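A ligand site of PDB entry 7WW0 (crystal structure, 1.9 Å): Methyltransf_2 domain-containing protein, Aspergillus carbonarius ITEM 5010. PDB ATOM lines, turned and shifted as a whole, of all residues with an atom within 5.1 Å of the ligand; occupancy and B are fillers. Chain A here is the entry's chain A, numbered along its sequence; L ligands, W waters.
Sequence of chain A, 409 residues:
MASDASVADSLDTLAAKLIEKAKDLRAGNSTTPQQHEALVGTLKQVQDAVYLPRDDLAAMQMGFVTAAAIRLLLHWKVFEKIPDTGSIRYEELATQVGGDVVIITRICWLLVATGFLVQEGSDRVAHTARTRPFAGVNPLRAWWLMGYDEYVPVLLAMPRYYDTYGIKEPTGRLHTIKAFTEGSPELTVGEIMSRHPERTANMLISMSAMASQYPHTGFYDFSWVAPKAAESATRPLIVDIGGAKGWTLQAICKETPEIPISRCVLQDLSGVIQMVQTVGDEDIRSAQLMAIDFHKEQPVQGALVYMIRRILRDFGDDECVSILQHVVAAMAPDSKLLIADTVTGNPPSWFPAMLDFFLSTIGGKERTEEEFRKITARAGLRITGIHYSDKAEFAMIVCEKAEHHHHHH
OD1 of Asp 268 sits at hydrogen-bond distance from O5 of the ligand, at 2.6 Å.
N1 of the ligand sits at hydrogen-bond distance from O of Gly 242 (2.8 Å).
O of Arg 309 is in hydrogen-bond range of N1 of the ligand, 3.0 Å away.
O2 of the ligand is in salt-bridge range of NE of Arg 309, 2.9 Å away.
The side-chain carboxylate (OD1) of Asp 293 lies within hydrogen-bond range of a nitrogen (N4) of the ligand (2.9 Å).
The backbone NH of Phe 294 sits at hydrogen-bond distance from a nitrogen (N5) of the ligand (3.1 Å).
Water W4 lies within hydrogen-bond range of O1 of the ligand (2.6 Å), O of Met 207 (2.9 Å), NH1 of Arg 310 (2.9 Å), NH2 of Arg 309 (3.0 Å) and NE2 of His 216 (3.4 Å).
Water W2 lies within hydrogen-bond range of a nitrogen (N1) of the ligand (2.7 Å), the side-chain carboxylate of Asp 240 (2.7 Å) and the side-chain hydroxyl of Thr 248 (3.4 Å).
Water W6 lies within hydrogen-bond range of a nitrogen (N3) of the ligand (2.7 Å), a ring nitrogen (NE2) of His 295 (2.8 Å) and the side-chain hydroxyl (OG1) of Thr 188 (2.9 Å).
Water W3 bridges O of Gly 190 (2.8 Å) and O5 of the ligand (2.8 Å).
Water W8 bridges OG1 of Thr 188 and N4 of the ligand.
Water W1 lies within hydrogen-bond range of the backbone carbonyl oxygen of Ile 241, the backbone NH of Arg 309, the side-chain carboxylate of Asp 240 and a nitrogen (N1) of the ligand.
S1 of the ligand lies close to SD of Met 207, 3.6 Å away.
Residues that only touch the ligand: Gly 190 (3.99 Å), Met 203 (3.9 Å), His 216 (3.9 Å), Gly 243 (3.7 Å), Ala 244 (3.6 Å), Leu 269 (3.4 Å), Val 272 (3.5 Å), Ile 292 (3.7 Å), His 295 (3.3 Å), Arg 310 (3.5 Å), Ile 311 (3.6 Å) and Asp 314 (3.9 Å).
Hydrophobic or aromatic side chains within 4 Å of the ligand: Met 203, Met 207, His 216, Ala 244, Leu 269, Val 272, Ile 292, Phe 294, His 295 and Ile 311.
Within 4 Å of the ligand: Gly 190, Met 203, Met 207, His 216, Gly 242, Gly 243, Ala 244, Asp 268, Leu 269, Val 272, Ile 292, Asp 293, Phe 294, His 295, Arg 309, Arg 310, Ile 311 and Asp 314.
The side-chain carboxylate of Asp 268 is in hydrogen-bond range of the backbone NH of Ala 244.
O of Asp 268 is in hydrogen-bond range of N of Ile 292 (2.9 Å).
O of Gln 267 sits at hydrogen-bond distance from N of Gly 242, at 2.8 Å.
The guanidinium group (NH2) of Arg 309 lies close to a ring nitrogen (NE2) of His 216, at 3.4 Å.
The side-chain hydroxyl (OG1) of Thr 248 lies close to the guanidinium group (NE) of Arg 309, at 3.4 Å.
N of His 295 lies within hydrogen-bond range of OD1 of Asp 293 (2.9 Å).
A ring nitrogen (NE2) of His 216 is in hydrogen-bond range of the backbone carbonyl oxygen of Met 207 (3.0 Å).
A ring nitrogen (ND1) of His 216 is in hydrogen-bond range of the side-chain hydroxyl (OG1) of Thr 248 (2.7 Å).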
ATOM      1  N   THR A 188     -28.332  32.777  29.847  1.00  0.00           N
ATOM      2  CA  THR A 188     -28.568  31.516  30.540  1.00  0.00           C
ATOM      3  C   THR A 188     -27.242  30.834  30.838  1.00  0.00           C
ATOM      4  O   THR A 188     -26.194  31.187  30.313  1.00  0.00           O
ATOM      5  CB  THR A 188     -29.445  30.569  29.716  1.00  0.00           C
ATOM      6  OG1 THR A 188     -28.669  30.102  28.612  1.00  0.00           O
ATOM      7  CG2 THR A 188     -30.722  31.265  29.170  1.00  0.00           C
ATOM      8  N   GLY A 190     -26.359  27.818  30.004  1.00  0.00           N
ATOM      9  CA  GLY A 190     -25.890  27.130  28.798  1.00  0.00           C
ATOM     10  C   GLY A 190     -25.199  28.067  27.842  1.00  0.00           C
ATOM     11  O   GLY A 190     -24.212  27.697  27.196  1.00  0.00           O
ATOM     12  N   MET A 203     -17.041  20.532  29.120  1.00  0.00           N
ATOM     13  CA  MET A 203     -18.433  20.155  29.360  1.00  0.00           C
ATOM     14  C   MET A 203     -18.838  18.989  28.455  1.00  0.00           C
ATOM     15  O   MET A 203     -19.443  18.025  28.924  1.00  0.00           O
ATOM     16  CB  MET A 203     -19.354  21.361  29.157  1.00  0.00           C
ATOM     17  CG  MET A 203     -20.864  21.035  29.377  1.00  0.00           C
ATOM     18  SD  MET A 203     -21.670  20.358  27.909  1.00  0.00           S
ATOM     19  CE  MET A 203     -21.616  21.827  26.840  1.00  0.00           C
ATOM     20  N   LEU A 204     -18.465  19.026  27.170  1.00  0.00           N
ATOM     21  CA  LEU A 204     -18.865  17.967  26.252  1.00  0.00           C
ATOM     22  C   LEU A 204     -18.300  16.626  26.680  1.00  0.00           C
ATOM     23  O   LEU A 204     -18.995  15.610  26.659  1.00  0.00           O
ATOM     24  CB  LEU A 204     -18.390  18.275  24.829  1.00  0.00           C
ATOM     25  CG  LEU A 204     -19.045  19.514  24.179  1.00  0.00           C
ATOM     26  CD1 LEU A 204     -18.384  19.747  22.838  1.00  0.00           C
ATOM     27  CD2 LEU A 204     -20.559  19.278  24.037  1.00  0.00           C
ATOM     28  N   MET A 207     -20.031  14.748  29.618  1.00  0.00           N
ATOM     29  CA  MET A 207     -21.342  14.138  29.476  1.00  0.00           C
ATOM     30  C   MET A 207     -21.276  12.616  29.314  1.00  0.00           C
ATOM     31  O   MET A 207     -22.313  11.964  29.410  1.00  0.00           O
ATOM     32  CB  MET A 207     -22.101  14.767  28.294  1.00  0.00           C
ATOM     33  CG  MET A 207     -22.516  16.212  28.535  1.00  0.00           C
ATOM     34  SD  MET A 207     -23.540  16.414  30.021  1.00  0.00           S
ATOM     35  CE  MET A 207     -22.802  17.891  30.680  1.00  0.00           C
ATOM     36  N   HIS A 216     -26.420   5.806  29.191  1.00  0.00           N
ATOM     37  CA  HIS A 216     -26.855   6.277  27.867  1.00  0.00           C
ATOM     38  C   HIS A 216     -27.704   5.253  27.110  1.00  0.00           C
ATOM     39  O   HIS A 216     -28.528   5.630  26.264  1.00  0.00           O
ATOM     40  CB  HIS A 216     -25.654   6.650  27.015  1.00  0.00           C
ATOM     41  CG  HIS A 216     -25.001   7.926  27.439  1.00  0.00           C
ATOM     42  ND1 HIS A 216     -25.269   9.139  26.839  1.00  0.00           N
ATOM     43  CD2 HIS A 216     -24.129   8.193  28.452  1.00  0.00           C
ATOM     44  CE1 HIS A 216     -24.572  10.099  27.443  1.00  0.00           C
ATOM     45  NE2 HIS A 216     -23.859   9.544  28.410  1.00  0.00           N
ATOM     46  N   ASP A 240     -32.039  14.919  18.771  1.00  0.00           N
ATOM     47  CA  ASP A 240     -31.390  14.963  20.086  1.00  0.00           C
ATOM     48  C   ASP A 240     -31.287  16.419  20.531  1.00  0.00           C
ATOM     49  O   ASP A 240     -30.406  17.160  20.082  1.00  0.00           O
ATOM     50  CB  ASP A 240     -30.029  14.290  19.955  1.00  0.00           C
ATOM     51  CG  ASP A 240     -29.383  13.955  21.289  1.00  0.00           C
ATOM     52  OD1 ASP A 240     -30.000  14.266  22.347  1.00  0.00           O
ATOM     53  OD2 ASP A 240     -28.244  13.412  21.261  1.00  0.00           O
ATOM     54  N   ILE A 241     -32.233  16.873  21.361  1.00  0.00           N
ATOM     55  CA  ILE A 241     -32.373  18.294  21.680  1.00  0.00           C
ATOM     56  C   ILE A 241     -31.445  18.623  22.844  1.00  0.00           C
ATOM     57  O   ILE A 241     -31.633  18.112  23.953  1.00  0.00           O
ATOM     58  CB  ILE A 241     -33.843  18.629  22.034  1.00  0.00           C
ATOM     59  CG1 ILE A 241     -34.780  18.250  20.865  1.00  0.00           C
ATOM     60  CG2 ILE A 241     -33.987  20.124  22.484  1.00  0.00           C
ATOM     61  CD1 ILE A 241     -36.248  18.378  21.266  1.00  0.00           C
ATOM     62  N   GLY A 242     -30.439  19.475  22.588  1.00  0.00           N
ATOM     63  CA  GLY A 242     -29.397  19.742  23.571  1.00  0.00           C
ATOM     64  C   GLY A 242     -28.536  18.501  23.745  1.00  0.00           C
ATOM     65  O   GLY A 242     -28.194  18.133  24.870  1.00  0.00           O
ATOM     66  N   GLY A 243     -28.153  17.887  22.633  1.00  0.00           N
ATOM     67  CA  GLY A 243     -27.480  16.602  22.689  1.00  0.00           C
ATOM     68  C   GLY A 243     -25.978  16.661  22.849  1.00  0.00           C
ATOM     69  O   GLY A 243     -25.350  15.594  22.815  1.00  0.00           O
ATOM     70  N   ALA A 244     -25.387  17.837  23.110  1.00  0.00           N
ATOM     71  CA  ALA A 244     -23.957  17.988  23.447  1.00  0.00           C
ATOM     72  C   ALA A 244     -23.158  17.489  22.236  1.00  0.00           C
ATOM     73  O   ALA A 244     -23.318  18.059  21.152  1.00  0.00           O
ATOM     74  CB  ALA A 244     -23.668  17.294  24.766  1.00  0.00           C
ATOM     75  N   THR A 248     -24.963  10.206  23.018  1.00  0.00           N
ATOM     76  CA  THR A 248     -26.119   9.351  23.202  1.00  0.00           C
ATOM     77  C   THR A 248     -26.651   8.844  21.864  1.00  0.00           C
ATOM     78  O   THR A 248     -27.059   7.684  21.772  1.00  0.00           O
ATOM     79  CB  THR A 248     -27.224  10.091  23.969  1.00  0.00           C
ATOM     80  OG1 THR A 248     -26.646  10.699  25.137  1.00  0.00           O
ATOM     81  CG2 THR A 248     -28.309   9.105  24.425  1.00  0.00           C
ATOM     82  N   GLN A 267     -28.878  18.666  17.945  1.00  0.00           N
ATOM     83  CA  GLN A 267     -29.136  20.088  18.111  1.00  0.00           C
ATOM     84  C   GLN A 267     -28.514  20.580  19.402  1.00  0.00           C
ATOM     85  O   GLN A 267     -28.644  19.933  20.442  1.00  0.00           O
ATOM     86  CB  GLN A 267     -30.626  20.363  18.199  1.00  0.00           C
ATOM     87  CG  GLN A 267     -31.369  20.029  16.884  1.00  0.00           C
ATOM     88  CD  GLN A 267     -32.867  20.139  17.030  1.00  0.00           C
ATOM     89  OE1 GLN A 267     -33.407  20.049  18.133  1.00  0.00           O
ATOM     90  NE2 GLN A 267     -33.568  20.378  15.887  1.00  0.00           N
ATOM     91  N   ASP A 268     -27.921  21.771  19.334  1.00  0.00           N
ATOM     92  CA  ASP A 268     -27.391  22.417  20.536  1.00  0.00           C
ATOM     93  C   ASP A 268     -27.193  23.899  20.222  1.00  0.00           C
ATOM     94  O   ASP A 268     -27.477  24.362  19.114  1.00  0.00           O
ATOM     95  CB  ASP A 268     -26.097  21.710  20.996  1.00  0.00           C
ATOM     96  CG  ASP A 268     -25.948  21.738  22.524  1.00  0.00           C
ATOM     97  OD1 ASP A 268     -25.742  22.845  23.042  1.00  0.00           O
ATOM     98  OD2 ASP A 268     -26.109  20.695  23.211  1.00  0.00           O
ATOM     99  N   LEU A 269     -26.709  24.666  21.217  1.00  0.00           N
ATOM    100  CA  LEU A 269     -26.353  26.073  20.973  1.00  0.00           C
ATOM    101  C   LEU A 269     -25.287  26.175  19.902  1.00  0.00           C
ATOM    102  O   LEU A 269     -24.400  25.318  19.780  1.00  0.00           O
ATOM    103  CB  LEU A 269     -25.803  26.725  22.253  1.00  0.00           C
ATOM    104  CG  LEU A 269     -26.906  26.793  23.330  1.00  0.00           C
ATOM    105  CD1 LEU A 269     -26.275  27.109  24.710  1.00  0.00           C
ATOM    106  CD2 LEU A 269     -27.921  27.824  22.948  1.00  0.00           C
ATOM    107  N   VAL A 272     -21.683  25.409  20.889  1.00  0.00           N
ATOM    108  CA  VAL A 272     -21.439  23.999  21.186  1.00  0.00           C
ATOM    109  C   VAL A 272     -21.409  23.185  19.901  1.00  0.00           C
ATOM    110  O   VAL A 272     -20.530  22.330  19.720  1.00  0.00           O
ATOM    111  CB  VAL A 272     -22.519  23.484  22.134  1.00  0.00           C
ATOM    112  CG1 VAL A 272     -22.462  21.979  22.296  1.00  0.00           C
ATOM    113  CG2 VAL A 272     -22.452  24.265  23.522  1.00  0.00           C
ATOM    114  N   ILE A 292     -29.632  25.490  17.483  1.00  0.00           N
ATOM    115  CA  ILE A 292     -30.982  25.883  17.876  1.00  0.00           C
ATOM    116  C   ILE A 292     -30.901  26.678  19.176  1.00  0.00           C
ATOM    117  O   ILE A 292     -29.848  26.780  19.793  1.00  0.00           O
ATOM    118  CB  ILE A 292     -31.931  24.672  18.106  1.00  0.00           C
ATOM    119  CG1 ILE A 292     -31.513  23.893  19.374  1.00  0.00           C
ATOM    120  CG2 ILE A 292     -31.983  23.713  16.866  1.00  0.00           C
ATOM    121  CD1 ILE A 292     -32.638  22.990  19.976  1.00  0.00           C
ATOM    122  N   ASP A 293     -32.043  27.200  19.594  1.00  0.00           N
ATOM    123  CA  ASP A 293     -32.228  27.688  20.967  1.00  0.00           C
ATOM    124  C   ASP A 293     -33.525  27.104  21.488  1.00  0.00           C
ATOM    125  O   ASP A 293     -34.619  27.580  21.130  1.00  0.00           O
ATOM    126  CB  ASP A 293     -32.235  29.214  21.014  1.00  0.00           C
ATOM    127  CG  ASP A 293     -32.463  29.743  22.443  1.00  0.00           C
ATOM    128  OD1 ASP A 293     -32.787  28.934  23.360  1.00  0.00           O
ATOM    129  OD2 ASP A 293     -32.294  30.967  22.619  1.00  0.00           O
ATOM    130  N   PHE A 294     -33.430  26.077  22.346  1.00  0.00           N
ATOM    131  CA  PHE A 294     -34.652  25.369  22.675  1.00  0.00           C
ATOM    132  C   PHE A 294     -35.573  26.161  23.602  1.00  0.00           C
ATOM    133  O   PHE A 294     -36.691  25.714  23.867  1.00  0.00           O
ATOM    134  CB  PHE A 294     -34.358  23.944  23.235  1.00  0.00           C
ATOM    135  CG  PHE A 294     -33.448  23.849  24.476  1.00  0.00           C
ATOM    136  CD1 PHE A 294     -33.671  24.590  25.648  1.00  0.00           C
ATOM    137  CD2 PHE A 294     -32.415  22.925  24.476  1.00  0.00           C
ATOM    138  CE1 PHE A 294     -32.820  24.421  26.790  1.00  0.00           C
ATOM    139  CE2 PHE A 294     -31.583  22.720  25.605  1.00  0.00           C
ATOM    140  CZ  PHE A 294     -31.767  23.468  26.762  1.00  0.00           C
ATOM    141  N   HIS A 295     -35.127  27.334  24.091  1.00  0.00           N
ATOM    142  CA  HIS A 295     -36.040  28.200  24.827  1.00  0.00           C
ATOM    143  C   HIS A 295     -37.025  28.872  23.890  1.00  0.00           C
ATOM    144  O   HIS A 295     -38.066  29.390  24.359  1.00  0.00           O
ATOM    145  CB  HIS A 295     -35.256  29.285  25.605  1.00  0.00           C
ATOM    146  CG  HIS A 295     -34.383  28.732  26.677  1.00  0.00           C
ATOM    147  ND1 HIS A 295     -34.868  27.944  27.694  1.00  0.00           N
ATOM    148  CD2 HIS A 295     -33.034  28.792  26.845  1.00  0.00           C
ATOM    149  CE1 HIS A 295     -33.858  27.586  28.477  1.00  0.00           C
ATOM    150  NE2 HIS A 295     -32.740  28.077  27.980  1.00  0.00           N
ATOM    151  N   ARG A 309     -32.825  14.765  26.783  1.00  0.00           N
ATOM    152  CA  ARG A 309     -32.031  13.988  27.715  1.00  0.00           C
ATOM    153  C   ARG A 309     -31.254  14.929  28.632  1.00  0.00           C
ATOM    154  O   ARG A 309     -30.443  15.738  28.154  1.00  0.00           O
ATOM    155  CB  ARG A 309     -31.068  13.069  26.965  1.00  0.00           C
ATOM    156  CG  ARG A 309     -30.147  12.256  27.933  1.00  0.00           C
ATOM    157  CD  ARG A 309     -29.016  11.531  27.205  1.00  0.00           C
ATOM    158  NE  ARG A 309     -27.940  11.239  28.182  1.00  0.00           N
ATOM    159  CZ  ARG A 309     -27.892  10.156  28.933  1.00  0.00           C
ATOM    160  NH1 ARG A 309     -28.826   9.231  28.807  1.00  0.00           N
ATOM    161  NH2 ARG A 309     -26.915  10.005  29.851  1.00  0.00           N
ATOM    162  N   ARG A 310     -31.494  14.834  29.931  1.00  0.00           N
ATOM    163  CA  ARG A 310     -30.789  15.634  30.936  1.00  0.00           C
ATOM    164  C   ARG A 310     -30.827  17.126  30.610  1.00  0.00           C
ATOM    165  O   ARG A 310     -29.830  17.850  30.759  1.00  0.00           O
ATOM    166  CB  ARG A 310     -29.356  15.128  31.091  1.00  0.00           C
ATOM    167  CG  ARG A 310     -29.339  13.619  31.392  1.00  0.00           C
ATOM    168  CD  ARG A 310     -27.912  13.135  31.731  1.00  0.00           C
ATOM    169  NE  ARG A 310     -27.477  13.762  32.975  1.00  0.00           N
ATOM    170  CZ  ARG A 310     -26.217  14.094  33.250  1.00  0.00           C
ATOM    171  NH1 ARG A 310     -25.262  13.862  32.364  1.00  0.00           N
ATOM    172  NH2 ARG A 310     -25.925  14.650  34.437  1.00  0.00           N
ATOM    173  N   ILE A 311     -31.984  17.576  30.149  1.00  0.00           N
ATOM    174  CA  ILE A 311     -32.280  18.971  29.893  1.00  0.00           C
ATOM    175  C   ILE A 311     -33.186  19.549  30.976  1.00  0.00           C
ATOM    176  O   ILE A 311     -32.906  20.610  31.534  1.00  0.00           O
ATOM    177  CB  ILE A 311     -32.924  19.153  28.508  1.00  0.00           C
ATOM    178  CG1 ILE A 311     -32.070  18.546  27.394  1.00  0.00           C
ATOM    179  CG2 ILE A 311     -33.285  20.665  28.299  1.00  0.00           C
ATOM    180  CD1 ILE A 311     -30.577  18.973  27.392  1.00  0.00           C
ATOM    181  N   ASP A 314     -32.136  21.098  34.325  1.00  0.00           N
ATOM    182  CA  ASP A 314     -31.438  22.379  34.347  1.00  0.00           C
ATOM    183  C   ASP A 314     -32.371  23.575  34.448  1.00  0.00           C
ATOM    184  O   ASP A 314     -31.878  24.718  34.473  1.00  0.00           O
ATOM    185  CB  ASP A 314     -30.574  22.542  33.074  1.00  0.00           C
ATOM    186  CG  ASP A 314     -29.396  21.553  33.036  1.00  0.00           C
ATOM    187  OD1 ASP A 314     -29.105  20.929  34.097  1.00  0.00           O
ATOM    188  OD2 ASP A 314     -28.792  21.395  31.948  1.00  0.00           O
ATOM    189  N   PHE A 315     -33.674  23.365  34.505  1.00  0.00           N
ATOM    190  CA  PHE A 315     -34.610  24.504  34.443  1.00  0.00           C
ATOM    191  C   PHE A 315     -35.760  24.309  35.415  1.00  0.00           C
ATOM    192  O   PHE A 315     -36.093  23.187  35.809  1.00  0.00           O
ATOM    193  CB  PHE A 315     -35.157  24.722  33.018  1.00  0.00           C
ATOM    194  CG  PHE A 315     -34.067  24.877  32.009  1.00  0.00           C
ATOM    195  CD1 PHE A 315     -33.404  26.109  31.897  1.00  0.00           C
ATOM    196  CD2 PHE A 315     -33.629  23.790  31.291  1.00  0.00           C
ATOM    197  CE1 PHE A 315     -32.313  26.253  31.032  1.00  0.00           C
ATOM    198  CE2 PHE A 315     -32.549  23.898  30.401  1.00  0.00           C
ATOM    199  CZ  PHE A 315     -31.891  25.132  30.276  1.00  0.00           C
HETATM  200  N1  LIG L   1     -28.152  15.618  26.199  1.00  0.00           N
HETATM  201  C1  LIG L   1     -26.724  15.560  26.607  1.00  0.00           C
HETATM  202  C2  LIG L   1     -26.277  16.886  27.239  1.00  0.00           C
HETATM  203  C3  LIG L   1     -26.994  17.349  28.496  1.00  0.00           C
HETATM  204  S1  LIG L   1     -26.101  18.811  29.167  1.00  0.00           S
HETATM  205  C4  LIG L   1     -26.484  14.444  27.623  1.00  0.00           C
HETATM  206  O1  LIG L   1     -25.383  13.868  27.728  1.00  0.00           O
HETATM  207  O2  LIG L   1     -27.415  14.069  28.335  1.00  0.00           O
HETATM  208  C5  LIG L   1     -27.223  20.144  28.612  1.00  0.00           C
HETATM  209  C6  LIG L   1     -27.071  20.495  27.109  1.00  0.00           C
HETATM  210  O3  LIG L   1     -28.043  21.513  26.769  1.00  0.00           O
HETATM  211  C7  LIG L   1     -25.705  21.125  26.793  1.00  0.00           C
HETATM  212  O4  LIG L   1     -25.059  20.502  25.706  1.00  0.00           O
HETATM  213  C8  LIG L   1     -26.042  22.595  26.459  1.00  0.00           C
HETATM  214  O5  LIG L   1     -25.105  23.193  25.553  1.00  0.00           O
HETATM  215  C9  LIG L   1     -27.426  22.443  25.873  1.00  0.00           C
HETATM  216  N2  LIG L   1     -28.199  23.685  25.918  1.00  0.00           N
HETATM  217  C10 LIG L   1     -28.347  24.568  26.978  1.00  0.00           C
HETATM  218  N3  LIG L   1     -29.177  25.591  26.605  1.00  0.00           N
HETATM  219  C11 LIG L   1     -29.538  25.347  25.308  1.00  0.00           C
HETATM  220  C12 LIG L   1     -30.382  26.017  24.446  1.00  0.00           C
HETATM  221  N4  LIG L   1     -31.006  27.135  24.796  1.00  0.00           N
HETATM  222  N5  LIG L   1     -30.561  25.485  23.202  1.00  0.00           N
HETATM  223  C13 LIG L   1     -29.935  24.327  22.782  1.00  0.00           C
HETATM  224  N6  LIG L   1     -29.100  23.647  23.639  1.00  0.00           N
HETATM  225  C14 LIG L   1     -28.949  24.148  24.888  1.00  0.00           C
HETATM  226  O   HOH W   1     -31.059  15.701  24.664  1.00  0.00           O
HETATM  227  O   HOH W   2     -28.383  13.597  24.461  1.00  0.00           O
HETATM  228  O   HOH W   3     -23.506  24.984  27.082  1.00  0.00           O
HETATM  229  O   HOH W   4     -25.116  12.375  29.876  1.00  0.00           O
HETATM  230  O   HOH W   5     -24.604  12.907  25.307  1.00  0.00           O
HETATM  231  O   HOH W   6     -29.988  27.582  28.306  1.00  0.00           O
HETATM  232  O   HOH W   7     -27.766  24.269  30.219  1.00  0.00           O
HETATM  233  O   HOH W   8     -29.839  30.050  25.758  1.00  0.00           O
